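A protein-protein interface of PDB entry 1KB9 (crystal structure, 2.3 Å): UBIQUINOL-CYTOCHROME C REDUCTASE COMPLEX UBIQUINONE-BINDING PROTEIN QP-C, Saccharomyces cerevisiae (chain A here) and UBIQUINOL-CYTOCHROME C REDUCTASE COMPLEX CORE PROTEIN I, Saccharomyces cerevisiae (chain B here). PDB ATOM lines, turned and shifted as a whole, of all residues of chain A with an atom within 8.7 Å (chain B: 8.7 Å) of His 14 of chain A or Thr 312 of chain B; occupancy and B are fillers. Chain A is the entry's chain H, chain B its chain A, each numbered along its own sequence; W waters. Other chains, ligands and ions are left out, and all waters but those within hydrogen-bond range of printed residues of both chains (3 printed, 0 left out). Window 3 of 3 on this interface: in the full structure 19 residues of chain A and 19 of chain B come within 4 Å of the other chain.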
ATOM      1  N   THR A   7     -40.694 -12.833  15.283  1.00  0.00           N
ATOM      2  CA  THR A   7     -40.516 -11.752  14.323  1.00  0.00           C
ATOM      3  C   THR A   7     -39.278 -12.010  13.460  1.00  0.00           C
ATOM      4  O   THR A   7     -38.681 -13.089  13.513  1.00  0.00           O
ATOM      5  CB  THR A   7     -40.344 -10.396  15.053  1.00  0.00           C
ATOM      6  OG1 THR A   7     -39.225 -10.468  15.947  1.00  0.00           O
ATOM      7  CG2 THR A   7     -41.596 -10.058  15.858  1.00  0.00           C
ATOM      8  N   TYR A   8     -38.890 -11.015  12.672  1.00  0.00           N
ATOM      9  CA  TYR A   8     -37.719 -11.148  11.815  1.00  0.00           C
ATOM     10  C   TYR A   8     -36.554 -10.287  12.296  1.00  0.00           C
ATOM     11  O   TYR A   8     -35.623 -10.012  11.543  1.00  0.00           O
ATOM     12  CB  TYR A   8     -38.085 -10.843  10.359  1.00  0.00           C
ATOM     13  CG  TYR A   8     -38.966 -11.910   9.751  1.00  0.00           C
ATOM     14  CD1 TYR A   8     -40.359 -11.771   9.721  1.00  0.00           C
ATOM     15  CD2 TYR A   8     -38.411 -13.083   9.254  1.00  0.00           C
ATOM     16  CE1 TYR A   8     -41.172 -12.782   9.215  1.00  0.00           C
ATOM     17  CE2 TYR A   8     -39.207 -14.095   8.748  1.00  0.00           C
ATOM     18  CZ  TYR A   8     -40.587 -13.945   8.731  1.00  0.00           C
ATOM     19  OH  TYR A   8     -41.355 -14.979   8.246  1.00  0.00           O
ATOM     20  N   MET A   9     -36.634  -9.845  13.549  1.00  0.00           N
ATOM     21  CA  MET A   9     -35.584  -9.043  14.171  1.00  0.00           C
ATOM     22  C   MET A   9     -35.527  -9.350  15.676  1.00  0.00           C
ATOM     23  O   MET A   9     -36.554  -9.408  16.342  1.00  0.00           O
ATOM     24  CB  MET A   9     -35.813  -7.537  13.955  1.00  0.00           C
ATOM     25  CG  MET A   9     -34.693  -6.681  14.545  1.00  0.00           C
ATOM     26  SD  MET A   9     -34.933  -4.895  14.446  1.00  0.00           S
ATOM     27  CE  MET A   9     -36.043  -4.602  15.816  1.00  0.00           C
ATOM     28  N   GLY A  10     -34.328  -9.615  16.181  1.00  0.00           N
ATOM     29  CA  GLY A  10     -34.157  -9.884  17.597  1.00  0.00           C
ATOM     30  C   GLY A  10     -33.532  -8.667  18.260  1.00  0.00           C
ATOM     31  O   GLY A  10     -33.955  -7.533  18.011  1.00  0.00           O
ATOM     32  N   TRP A  11     -32.502  -8.886  19.069  1.00  0.00           N
ATOM     33  CA  TRP A  11     -31.827  -7.784  19.751  1.00  0.00           C
ATOM     34  C   TRP A  11     -30.353  -8.128  19.833  1.00  0.00           C
ATOM     35  O   TRP A  11     -29.962  -9.221  19.455  1.00  0.00           O
ATOM     36  CB  TRP A  11     -32.410  -7.576  21.159  1.00  0.00           C
ATOM     37  CG  TRP A  11     -32.283  -6.153  21.669  1.00  0.00           C
ATOM     38  CD1 TRP A  11     -31.387  -5.679  22.601  1.00  0.00           C
ATOM     39  CD2 TRP A  11     -33.093  -5.030  21.286  1.00  0.00           C
ATOM     40  NE1 TRP A  11     -31.602  -4.336  22.819  1.00  0.00           N
ATOM     41  CE2 TRP A  11     -32.640  -3.913  22.030  1.00  0.00           C
ATOM     42  CE3 TRP A  11     -34.161  -4.861  20.391  1.00  0.00           C
ATOM     43  CZ2 TRP A  11     -33.222  -2.645  21.906  1.00  0.00           C
ATOM     44  CZ3 TRP A  11     -34.742  -3.599  20.268  1.00  0.00           C
ATOM     45  CH2 TRP A  11     -34.268  -2.508  21.025  1.00  0.00           C
ATOM     46  N   TRP A  12     -29.541  -7.199  20.326  1.00  0.00           N
ATOM     47  CA  TRP A  12     -28.100  -7.408  20.459  1.00  0.00           C
ATOM     48  C   TRP A  12     -27.760  -8.771  21.057  1.00  0.00           C
ATOM     49  O   TRP A  12     -28.175  -9.092  22.180  1.00  0.00           O
ATOM     50  CB  TRP A  12     -27.499  -6.300  21.313  1.00  0.00           C
ATOM     51  CG  TRP A  12     -27.750  -4.948  20.739  1.00  0.00           C
ATOM     52  CD1 TRP A  12     -28.590  -4.000  21.225  1.00  0.00           C
ATOM     53  CD2 TRP A  12     -27.149  -4.392  19.563  1.00  0.00           C
ATOM     54  NE1 TRP A  12     -28.555  -2.883  20.430  1.00  0.00           N
ATOM     55  CE2 TRP A  12     -27.675  -3.095  19.403  1.00  0.00           C
ATOM     56  CE3 TRP A  12     -26.214  -4.866  18.629  1.00  0.00           C
ATOM     57  CZ2 TRP A  12     -27.293  -2.250  18.343  1.00  0.00           C
ATOM     58  CZ3 TRP A  12     -25.833  -4.028  17.577  1.00  0.00           C
ATOM     59  CH2 TRP A  12     -26.371  -2.735  17.445  1.00  0.00           C
ATOM     60  N   GLY A  13     -27.043  -9.587  20.283  1.00  0.00           N
ATOM     61  CA  GLY A  13     -26.683 -10.915  20.745  1.00  0.00           C
ATOM     62  C   GLY A  13     -27.535 -12.003  20.108  1.00  0.00           C
ATOM     63  O   GLY A  13     -27.149 -13.176  20.117  1.00  0.00           O
ATOM     64  N   HIS A  14     -28.703 -11.633  19.582  1.00  0.00           N
ATOM     65  CA  HIS A  14     -29.604 -12.578  18.914  1.00  0.00           C
ATOM     66  C   HIS A  14     -30.453 -11.823  17.883  1.00  0.00           C
ATOM     67  O   HIS A  14     -31.684 -11.898  17.885  1.00  0.00           O
ATOM     68  CB  HIS A  14     -30.480 -13.330  19.938  1.00  0.00           C
ATOM     69  CG  HIS A  14     -31.322 -12.440  20.802  1.00  0.00           C
ATOM     70  ND1 HIS A  14     -32.673 -12.256  20.589  1.00  0.00           N
ATOM     71  CD2 HIS A  14     -31.004 -11.666  21.868  1.00  0.00           C
ATOM     72  CE1 HIS A  14     -33.149 -11.406  21.482  1.00  0.00           C
ATOM     73  NE2 HIS A  14     -32.157 -11.032  22.270  1.00  0.00           N
ATOM     74  N   MET A  15     -29.770 -11.109  16.989  1.00  0.00           N
ATOM     75  CA  MET A  15     -30.431 -10.293  15.977  1.00  0.00           C
ATOM     76  C   MET A  15     -31.304 -11.070  15.012  1.00  0.00           C
ATOM     77  O   MET A  15     -32.249 -10.515  14.445  1.00  0.00           O
ATOM     78  CB  MET A  15     -29.412  -9.468  15.195  1.00  0.00           C
ATOM     79  CG  MET A  15     -29.957  -8.137  14.704  1.00  0.00           C
ATOM     80  SD  MET A  15     -30.412  -7.044  16.069  1.00  0.00           S
ATOM     81  CE  MET A  15     -28.796  -6.478  16.600  1.00  0.00           C
ATOM     82  N   GLY A  16     -30.986 -12.350  14.829  1.00  0.00           N
ATOM     83  CA  GLY A  16     -31.760 -13.184  13.928  1.00  0.00           C
ATOM     84  C   GLY A  16     -31.101 -13.402  12.575  1.00  0.00           C
ATOM     85  O   GLY A  16     -31.697 -14.002  11.678  1.00  0.00           O
ATOM     86  N   GLY A  17     -29.889 -12.879  12.411  1.00  0.00           N
ATOM     87  CA  GLY A  17     -29.170 -13.061  11.168  1.00  0.00           C
ATOM     88  C   GLY A  17     -28.524 -14.433  11.134  1.00  0.00           C
ATOM     89  O   GLY A  17     -28.649 -15.204  12.094  1.00  0.00           O
ATOM     90  N   ARG B 226     -15.329 -11.517  14.586  1.00  0.00           N
ATOM     91  CA  ARG B 226     -16.573 -12.226  14.862  1.00  0.00           C
ATOM     92  C   ARG B 226     -16.575 -13.656  14.371  1.00  0.00           C
ATOM     93  O   ARG B 226     -16.123 -13.940  13.270  1.00  0.00           O
ATOM     94  CB  ARG B 226     -17.798 -11.497  14.292  1.00  0.00           C
ATOM     95  CG  ARG B 226     -19.033 -11.737  15.161  1.00  0.00           C
ATOM     96  CD  ARG B 226     -20.312 -11.990  14.396  1.00  0.00           C
ATOM     97  NE  ARG B 226     -21.155 -10.808  14.329  1.00  0.00           N
ATOM     98  CZ  ARG B 226     -22.485 -10.815  14.295  1.00  0.00           C
ATOM     99  NH1 ARG B 226     -23.128  -9.663  14.229  1.00  0.00           N
ATOM    100  NH2 ARG B 226     -23.177 -11.947  14.344  1.00  0.00           N
ATOM    101  N   ASP B 228     -19.511 -16.608  15.142  1.00  0.00           N
ATOM    102  CA  ASP B 228     -20.693 -17.088  15.849  1.00  0.00           C
ATOM    103  C   ASP B 228     -20.675 -18.573  16.196  1.00  0.00           C
ATOM    104  O   ASP B 228     -21.558 -19.046  16.916  1.00  0.00           O
ATOM    105  CB  ASP B 228     -21.972 -16.771  15.054  1.00  0.00           C
ATOM    106  CG  ASP B 228     -22.218 -15.281  14.883  1.00  0.00           C
ATOM    107  OD1 ASP B 228     -21.546 -14.466  15.540  1.00  0.00           O
ATOM    108  OD2 ASP B 228     -23.098 -14.917  14.081  1.00  0.00           O
ATOM    109  N   ALA B 233     -17.565 -15.246  23.964  1.00  0.00           N
ATOM    110  CA  ALA B 233     -17.058 -14.002  23.406  1.00  0.00           C
ATOM    111  C   ALA B 233     -15.837 -13.671  24.256  1.00  0.00           C
ATOM    112  O   ALA B 233     -15.894 -13.737  25.487  1.00  0.00           O
ATOM    113  CB  ALA B 233     -18.077 -12.891  23.508  1.00  0.00           C
ATOM    114  N   TYR B 283     -26.266 -10.666  37.314  1.00  0.00           N
ATOM    115  CA  TYR B 283     -26.722 -11.371  36.115  1.00  0.00           C
ATOM    116  C   TYR B 283     -25.601 -12.213  35.494  1.00  0.00           C
ATOM    117  O   TYR B 283     -25.771 -12.791  34.422  1.00  0.00           O
ATOM    118  CB  TYR B 283     -27.278 -10.381  35.079  1.00  0.00           C
ATOM    119  CG  TYR B 283     -28.614  -9.771  35.469  1.00  0.00           C
ATOM    120  CD1 TYR B 283     -28.674  -8.616  36.250  1.00  0.00           C
ATOM    121  CD2 TYR B 283     -29.820 -10.375  35.089  1.00  0.00           C
ATOM    122  CE1 TYR B 283     -29.893  -8.080  36.650  1.00  0.00           C
ATOM    123  CE2 TYR B 283     -31.051  -9.841  35.484  1.00  0.00           C
ATOM    124  CZ  TYR B 283     -31.078  -8.693  36.269  1.00  0.00           C
ATOM    125  OH  TYR B 283     -32.283  -8.160  36.688  1.00  0.00           O
ATOM    126  N   LEU B 285     -22.358 -11.420  34.306  1.00  0.00           N
ATOM    127  CA  LEU B 285     -21.882 -10.785  33.091  1.00  0.00           C
ATOM    128  C   LEU B 285     -20.658 -11.411  32.433  1.00  0.00           C
ATOM    129  O   LEU B 285     -20.318 -11.056  31.309  1.00  0.00           O
ATOM    130  CB  LEU B 285     -21.632  -9.300  33.377  1.00  0.00           C
ATOM    131  CG  LEU B 285     -22.850  -8.367  33.320  1.00  0.00           C
ATOM    132  CD1 LEU B 285     -24.090  -9.040  33.842  1.00  0.00           C
ATOM    133  CD2 LEU B 285     -22.565  -7.091  34.068  1.00  0.00           C
ATOM    134  N   THR B 308     -16.887 -14.455  28.191  1.00  0.00           N
ATOM    135  CA  THR B 308     -18.280 -14.571  28.629  1.00  0.00           C
ATOM    136  C   THR B 308     -19.233 -15.390  27.747  1.00  0.00           C
ATOM    137  O   THR B 308     -19.089 -15.444  26.530  1.00  0.00           O
ATOM    138  CB  THR B 308     -18.910 -13.167  28.825  1.00  0.00           C
ATOM    139  OG1 THR B 308     -20.275 -13.312  29.232  1.00  0.00           O
ATOM    140  CG2 THR B 308     -18.863 -12.362  27.535  1.00  0.00           C
ATOM    141  N   ARG B 309     -20.217 -16.013  28.385  1.00  0.00           N
ATOM    142  CA  ARG B 309     -21.239 -16.785  27.684  1.00  0.00           C
ATOM    143  C   ARG B 309     -22.561 -16.007  27.703  1.00  0.00           C
ATOM    144  O   ARG B 309     -23.571 -16.452  27.147  1.00  0.00           O
ATOM    145  CB  ARG B 309     -21.440 -18.148  28.342  1.00  0.00           C
ATOM    146  CG  ARG B 309     -20.373 -19.154  27.993  1.00  0.00           C
ATOM    147  CD  ARG B 309     -19.959 -19.968  29.204  1.00  0.00           C
ATOM    148  NE  ARG B 309     -21.088 -20.585  29.884  1.00  0.00           N
ATOM    149  CZ  ARG B 309     -21.434 -20.330  31.143  1.00  0.00           C
ATOM    150  NH1 ARG B 309     -22.482 -20.941  31.685  1.00  0.00           N
ATOM    151  NH2 ARG B 309     -20.743 -19.456  31.859  1.00  0.00           N
ATOM    152  N   ASN B 310     -22.552 -14.866  28.386  1.00  0.00           N
ATOM    153  CA  ASN B 310     -23.732 -14.025  28.474  1.00  0.00           C
ATOM    154  C   ASN B 310     -23.620 -13.075  27.290  1.00  0.00           C
ATOM    155  O   ASN B 310     -23.262 -11.896  27.424  1.00  0.00           O
ATOM    156  CB  ASN B 310     -23.752 -13.268  29.799  1.00  0.00           C
ATOM    157  CG  ASN B 310     -25.107 -12.661  30.099  1.00  0.00           C
ATOM    158  OD1 ASN B 310     -25.425 -12.368  31.252  1.00  0.00           O
ATOM    159  ND2 ASN B 310     -25.913 -12.464  29.062  1.00  0.00           N
ATOM    160  N   VAL B 311     -23.969 -13.604  26.124  1.00  0.00           N
ATOM    161  CA  VAL B 311     -23.848 -12.864  24.886  1.00  0.00           C
ATOM    162  C   VAL B 311     -24.831 -11.734  24.614  1.00  0.00           C
ATOM    163  O   VAL B 311     -24.580 -10.909  23.740  1.00  0.00           O
ATOM    164  CB  VAL B 311     -23.746 -13.826  23.689  1.00  0.00           C
ATOM    165  CG1 VAL B 311     -22.529 -14.719  23.877  1.00  0.00           C
ATOM    166  CG2 VAL B 311     -25.015 -14.658  23.551  1.00  0.00           C
ATOM    167  N   THR B 312     -25.897 -11.651  25.401  1.00  0.00           N
ATOM    168  CA  THR B 312     -26.886 -10.592  25.223  1.00  0.00           C
ATOM    169  C   THR B 312     -26.716  -9.447  26.216  1.00  0.00           C
ATOM    170  O   THR B 312     -27.522  -8.517  26.231  1.00  0.00           O
ATOM    171  CB  THR B 312     -28.325 -11.126  25.360  1.00  0.00           C
ATOM    172  OG1 THR B 312     -28.503 -11.719  26.652  1.00  0.00           O
ATOM    173  CG2 THR B 312     -28.615 -12.154  24.287  1.00  0.00           C
ATOM    174  N   MET B 313     -25.681  -9.522  27.052  1.00  0.00           N
ATOM    175  CA  MET B 313     -25.431  -8.493  28.055  1.00  0.00           C
ATOM    176  C   MET B 313     -23.992  -7.996  28.063  1.00  0.00           C
ATOM    177  O   MET B 313     -23.542  -7.379  29.025  1.00  0.00           O
ATOM    178  CB  MET B 313     -25.836  -8.994  29.443  1.00  0.00           C
ATOM    179  CG  MET B 313     -27.314  -9.330  29.545  1.00  0.00           C
ATOM    180  SD  MET B 313     -27.876  -9.819  31.163  1.00  0.00           S
ATOM    181  CE  MET B 313     -27.968  -8.201  31.963  1.00  0.00           C
ATOM    182  N   ILE B 314     -23.283  -8.240  26.969  1.00  0.00           N
ATOM    183  CA  ILE B 314     -21.904  -7.801  26.838  1.00  0.00           C
ATOM    184  C   ILE B 314     -21.806  -6.293  27.055  1.00  0.00           C
ATOM    185  O   ILE B 314     -20.821  -5.815  27.615  1.00  0.00           O
ATOM    186  CB  ILE B 314     -21.334  -8.177  25.449  1.00  0.00           C
ATOM    187  CG1 ILE B 314     -21.317  -9.693  25.284  1.00  0.00           C
ATOM    188  CG2 ILE B 314     -19.952  -7.650  25.278  1.00  0.00           C
ATOM    189  CD1 ILE B 314     -20.878 -10.140  23.912  1.00  0.00           C
ATOM    190  N   ASP B 315     -22.836  -5.546  26.655  1.00  0.00           N
ATOM    191  CA  ASP B 315     -22.805  -4.099  26.827  1.00  0.00           C
ATOM    192  C   ASP B 315     -22.784  -3.688  28.301  1.00  0.00           C
ATOM    193  O   ASP B 315     -22.195  -2.665  28.649  1.00  0.00           O
ATOM    194  CB  ASP B 315     -23.933  -3.388  26.042  1.00  0.00           C
ATOM    195  CG  ASP B 315     -25.331  -3.825  26.460  1.00  0.00           C
ATOM    196  OD1 ASP B 315     -25.649  -5.029  26.356  1.00  0.00           O
ATOM    197  OD2 ASP B 315     -26.128  -2.958  26.871  1.00  0.00           O
ATOM    198  N   ASP B 316     -23.399  -4.491  29.165  1.00  0.00           N
ATOM    199  CA  ASP B 316     -23.393  -4.189  30.593  1.00  0.00           C
ATOM    200  C   ASP B 316     -22.029  -4.506  31.200  1.00  0.00           C
ATOM    201  O   ASP B 316     -21.538  -3.771  32.062  1.00  0.00           O
ATOM    202  CB  ASP B 316     -24.515  -4.927  31.324  1.00  0.00           C
ATOM    203  CG  ASP B 316     -25.896  -4.386  30.961  1.00  0.00           C
ATOM    204  OD1 ASP B 316     -26.790  -5.189  30.633  1.00  0.00           O
ATOM    205  OD2 ASP B 316     -26.076  -3.151  30.988  1.00  0.00           O
ATOM    206  N   LEU B 317     -21.388  -5.554  30.688  1.00  0.00           N
ATOM    207  CA  LEU B 317     -20.067  -5.954  31.151  1.00  0.00           C
ATOM    208  C   LEU B 317     -19.117  -4.786  30.906  1.00  0.00           C
ATOM    209  O   LEU B 317     -18.463  -4.303  31.836  1.00  0.00           O
ATOM    210  CB  LEU B 317     -19.578  -7.168  30.366  1.00  0.00           C
ATOM    211  CG  LEU B 317     -18.554  -8.133  30.979  1.00  0.00           C
ATOM    212  CD1 LEU B 317     -17.867  -8.888  29.844  1.00  0.00           C
ATOM    213  CD2 LEU B 317     -17.518  -7.418  31.843  1.00  0.00           C
ATOM    214  N   GLN B 412     -18.797 -14.833  19.743  1.00  0.00           N
ATOM    215  CA  GLN B 412     -20.105 -14.198  19.615  1.00  0.00           C
ATOM    216  C   GLN B 412     -20.109 -12.758  20.127  1.00  0.00           C
ATOM    217  O   GLN B 412     -20.693 -12.471  21.173  1.00  0.00           O
ATOM    218  CB  GLN B 412     -21.160 -15.020  20.359  1.00  0.00           C
ATOM    219  CG  GLN B 412     -21.420 -16.369  19.734  1.00  0.00           C
ATOM    220  CD  GLN B 412     -22.439 -17.182  20.495  1.00  0.00           C
ATOM    221  OE1 GLN B 412     -22.148 -18.288  20.948  1.00  0.00           O
ATOM    222  NE2 GLN B 412     -23.647 -16.652  20.627  1.00  0.00           N
ATOM    223  N   ILE B 413     -19.474 -11.860  19.377  1.00  0.00           N
ATOM    224  CA  ILE B 413     -19.389 -10.454  19.762  1.00  0.00           C
ATOM    225  C   ILE B 413     -20.402  -9.507  19.088  1.00  0.00           C
ATOM    226  O   ILE B 413     -20.140  -8.308  18.941  1.00  0.00           O
ATOM    227  CB  ILE B 413     -17.958  -9.899  19.566  1.00  0.00           C
ATOM    228  CG1 ILE B 413     -17.469 -10.162  18.141  1.00  0.00           C
ATOM    229  CG2 ILE B 413     -17.007 -10.539  20.564  1.00  0.00           C
ATOM    230  CD1 ILE B 413     -16.144  -9.496  17.819  1.00  0.00           C
ATOM    231  N   GLU B 414     -21.547 -10.038  18.668  1.00  0.00           N
ATOM    232  CA  GLU B 414     -22.569  -9.192  18.059  1.00  0.00           C
ATOM    233  C   GLU B 414     -23.046  -8.151  19.092  1.00  0.00           C
ATOM    234  O   GLU B 414     -23.323  -7.000  18.751  1.00  0.00           O
ATOM    235  CB  GLU B 414     -23.758 -10.033  17.577  1.00  0.00           C
ATOM    236  CG  GLU B 414     -24.893  -9.217  16.956  1.00  0.00           C
ATOM    237  CD  GLU B 414     -26.075 -10.079  16.560  1.00  0.00           C
ATOM    238  OE1 GLU B 414     -26.935 -10.353  17.421  1.00  0.00           O
ATOM    239  OE2 GLU B 414     -26.145 -10.487  15.383  1.00  0.00           O
ATOM    240  N   GLY B 415     -23.083  -8.564  20.357  1.00  0.00           N
ATOM    241  CA  GLY B 415     -23.519  -7.693  21.429  1.00  0.00           C
ATOM    242  C   GLY B 415     -22.522  -6.634  21.879  1.00  0.00           C
ATOM    243  O   GLY B 415     -22.853  -5.796  22.722  1.00  0.00           O
ATOM    244  N   LEU B 416     -21.291  -6.698  21.376  1.00  0.00           N
ATOM    245  CA  LEU B 416     -20.277  -5.713  21.734  1.00  0.00           C
ATOM    246  C   LEU B 416     -20.630  -4.514  20.878  1.00  0.00           C
ATOM    247  O   LEU B 416     -20.621  -4.598  19.658  1.00  0.00           O
ATOM    248  CB  LEU B 416     -18.868  -6.233  21.404  1.00  0.00           C
ATOM    249  CG  LEU B 416     -17.680  -5.296  21.675  1.00  0.00           C
ATOM    250  CD1 LEU B 416     -17.480  -5.122  23.169  1.00  0.00           C
ATOM    251  CD2 LEU B 416     -16.410  -5.836  21.035  1.00  0.00           C
ATOM    252  N   LEU B 417     -21.030  -3.426  21.514  1.00  0.00           N
ATOM    253  CA  LEU B 417     -21.432  -2.232  20.778  1.00  0.00           C
ATOM    254  C   LEU B 417     -20.313  -1.550  19.993  1.00  0.00           C
ATOM    255  O   LEU B 417     -19.144  -1.898  20.122  1.00  0.00           O
ATOM    256  CB  LEU B 417     -22.111  -1.247  21.732  1.00  0.00           C
ATOM    257  CG  LEU B 417     -23.641  -1.341  21.865  1.00  0.00           C
ATOM    258  CD1 LEU B 417     -24.141  -2.755  21.656  1.00  0.00           C
ATOM    259  CD2 LEU B 417     -24.093  -0.778  23.203  1.00  0.00           C
HETATM  260  O   HOH W   1     -24.529 -14.243  19.511  1.00  0.00           O
HETATM  261  O   HOH W   2     -29.654  -7.909  24.285  1.00  0.00           O
HETATM  262  O   HOH W   3     -27.539 -12.482  14.016  1.00  0.00           O
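OE1 of Glu 414 of chain B is in hydrogen-bond range of N of His 14 of chain A (3.1 Å). OE1 of Glu 414 of chain B sits at hydrogen-bond distance from N of Gly 13 of chain A. The side-chain carboxylate of Glu 414 of chain B is in hydrogen-bond range of the backbone NH of Met 15 of chain A (3.0 Å).
N of Gly 10 of chain A lies within hydrogen-bond range of O of Met 15 of chain A (2.9 Å). The guanidinium group (NH1) of Arg 226 of chain B lies within salt-bridge range of the side-chain carboxylate (OE2) of Glu 414 of chain B, 3.3 Å away.
Among the printed residues, pairs that only touch across the chains: Trp 11 of chain A with Glu 414 of chain B, Trp 12 of chain A with Thr 312 of chain B, Trp 12 of chain A with Glu 414 of chain B, Gly 13 of chain A with Val 311 of chain B and His 14 of chain A with Thr 312 of chain B.
Of the printed residues of chain B, His 14 of chain A touches Thr 312 and Glu 414. Printed residues of chain A within 4 Å of Thr 312 of chain B: Trp 12 and His 14. Printed residues of chain B within 4 Å of Trp 11 of chain A: Glu 414. Printed residues of chain A within 4 Å of Val 311 of chain B: Gly 13. Thr 7 of chain A touches none of the printed residues of chain B. Tyr 8 of chain A touches none of the printed residues of chain B. The nearest printed residue of chain B that does not touch Met 15 of chain A is Arg 226 of chain B (6.4 Å).
Of the 11 printed residues of chain A, 5 touch a printed residue of chain B. Along chain A the printed residues that touch a printed residue of chain B span positions 11 to 15. Printed residues of chain B that touch a printed residue of chain A: Val 311, Thr 312 and Glu 414. Along chain B the printed residues that touch a printed residue of chain A span positions 311 to 414. Among the printed residues, 8 pairs touch across the chains. Among the printed residues, no Asp or Glu carboxylate lies within 4 Å of a Lys or Arg side-chain nitrogen of the other chain.
Water W3 bridges the side-chain carboxylate of Glu 414 of chain B (2.8 Å) and the backbone NH of Gly 17 of chain A (2.9 Å). Water W1 bridges NE2 of Gln 412 of chain B (2.8 Å) and O of Gly 13 of chain A (2.9 Å). Water W2 lies within hydrogen-bond range of O of Trp 12 of chain A (2.8 Å) and O of Thr 312 of chain B (2.9 Å).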
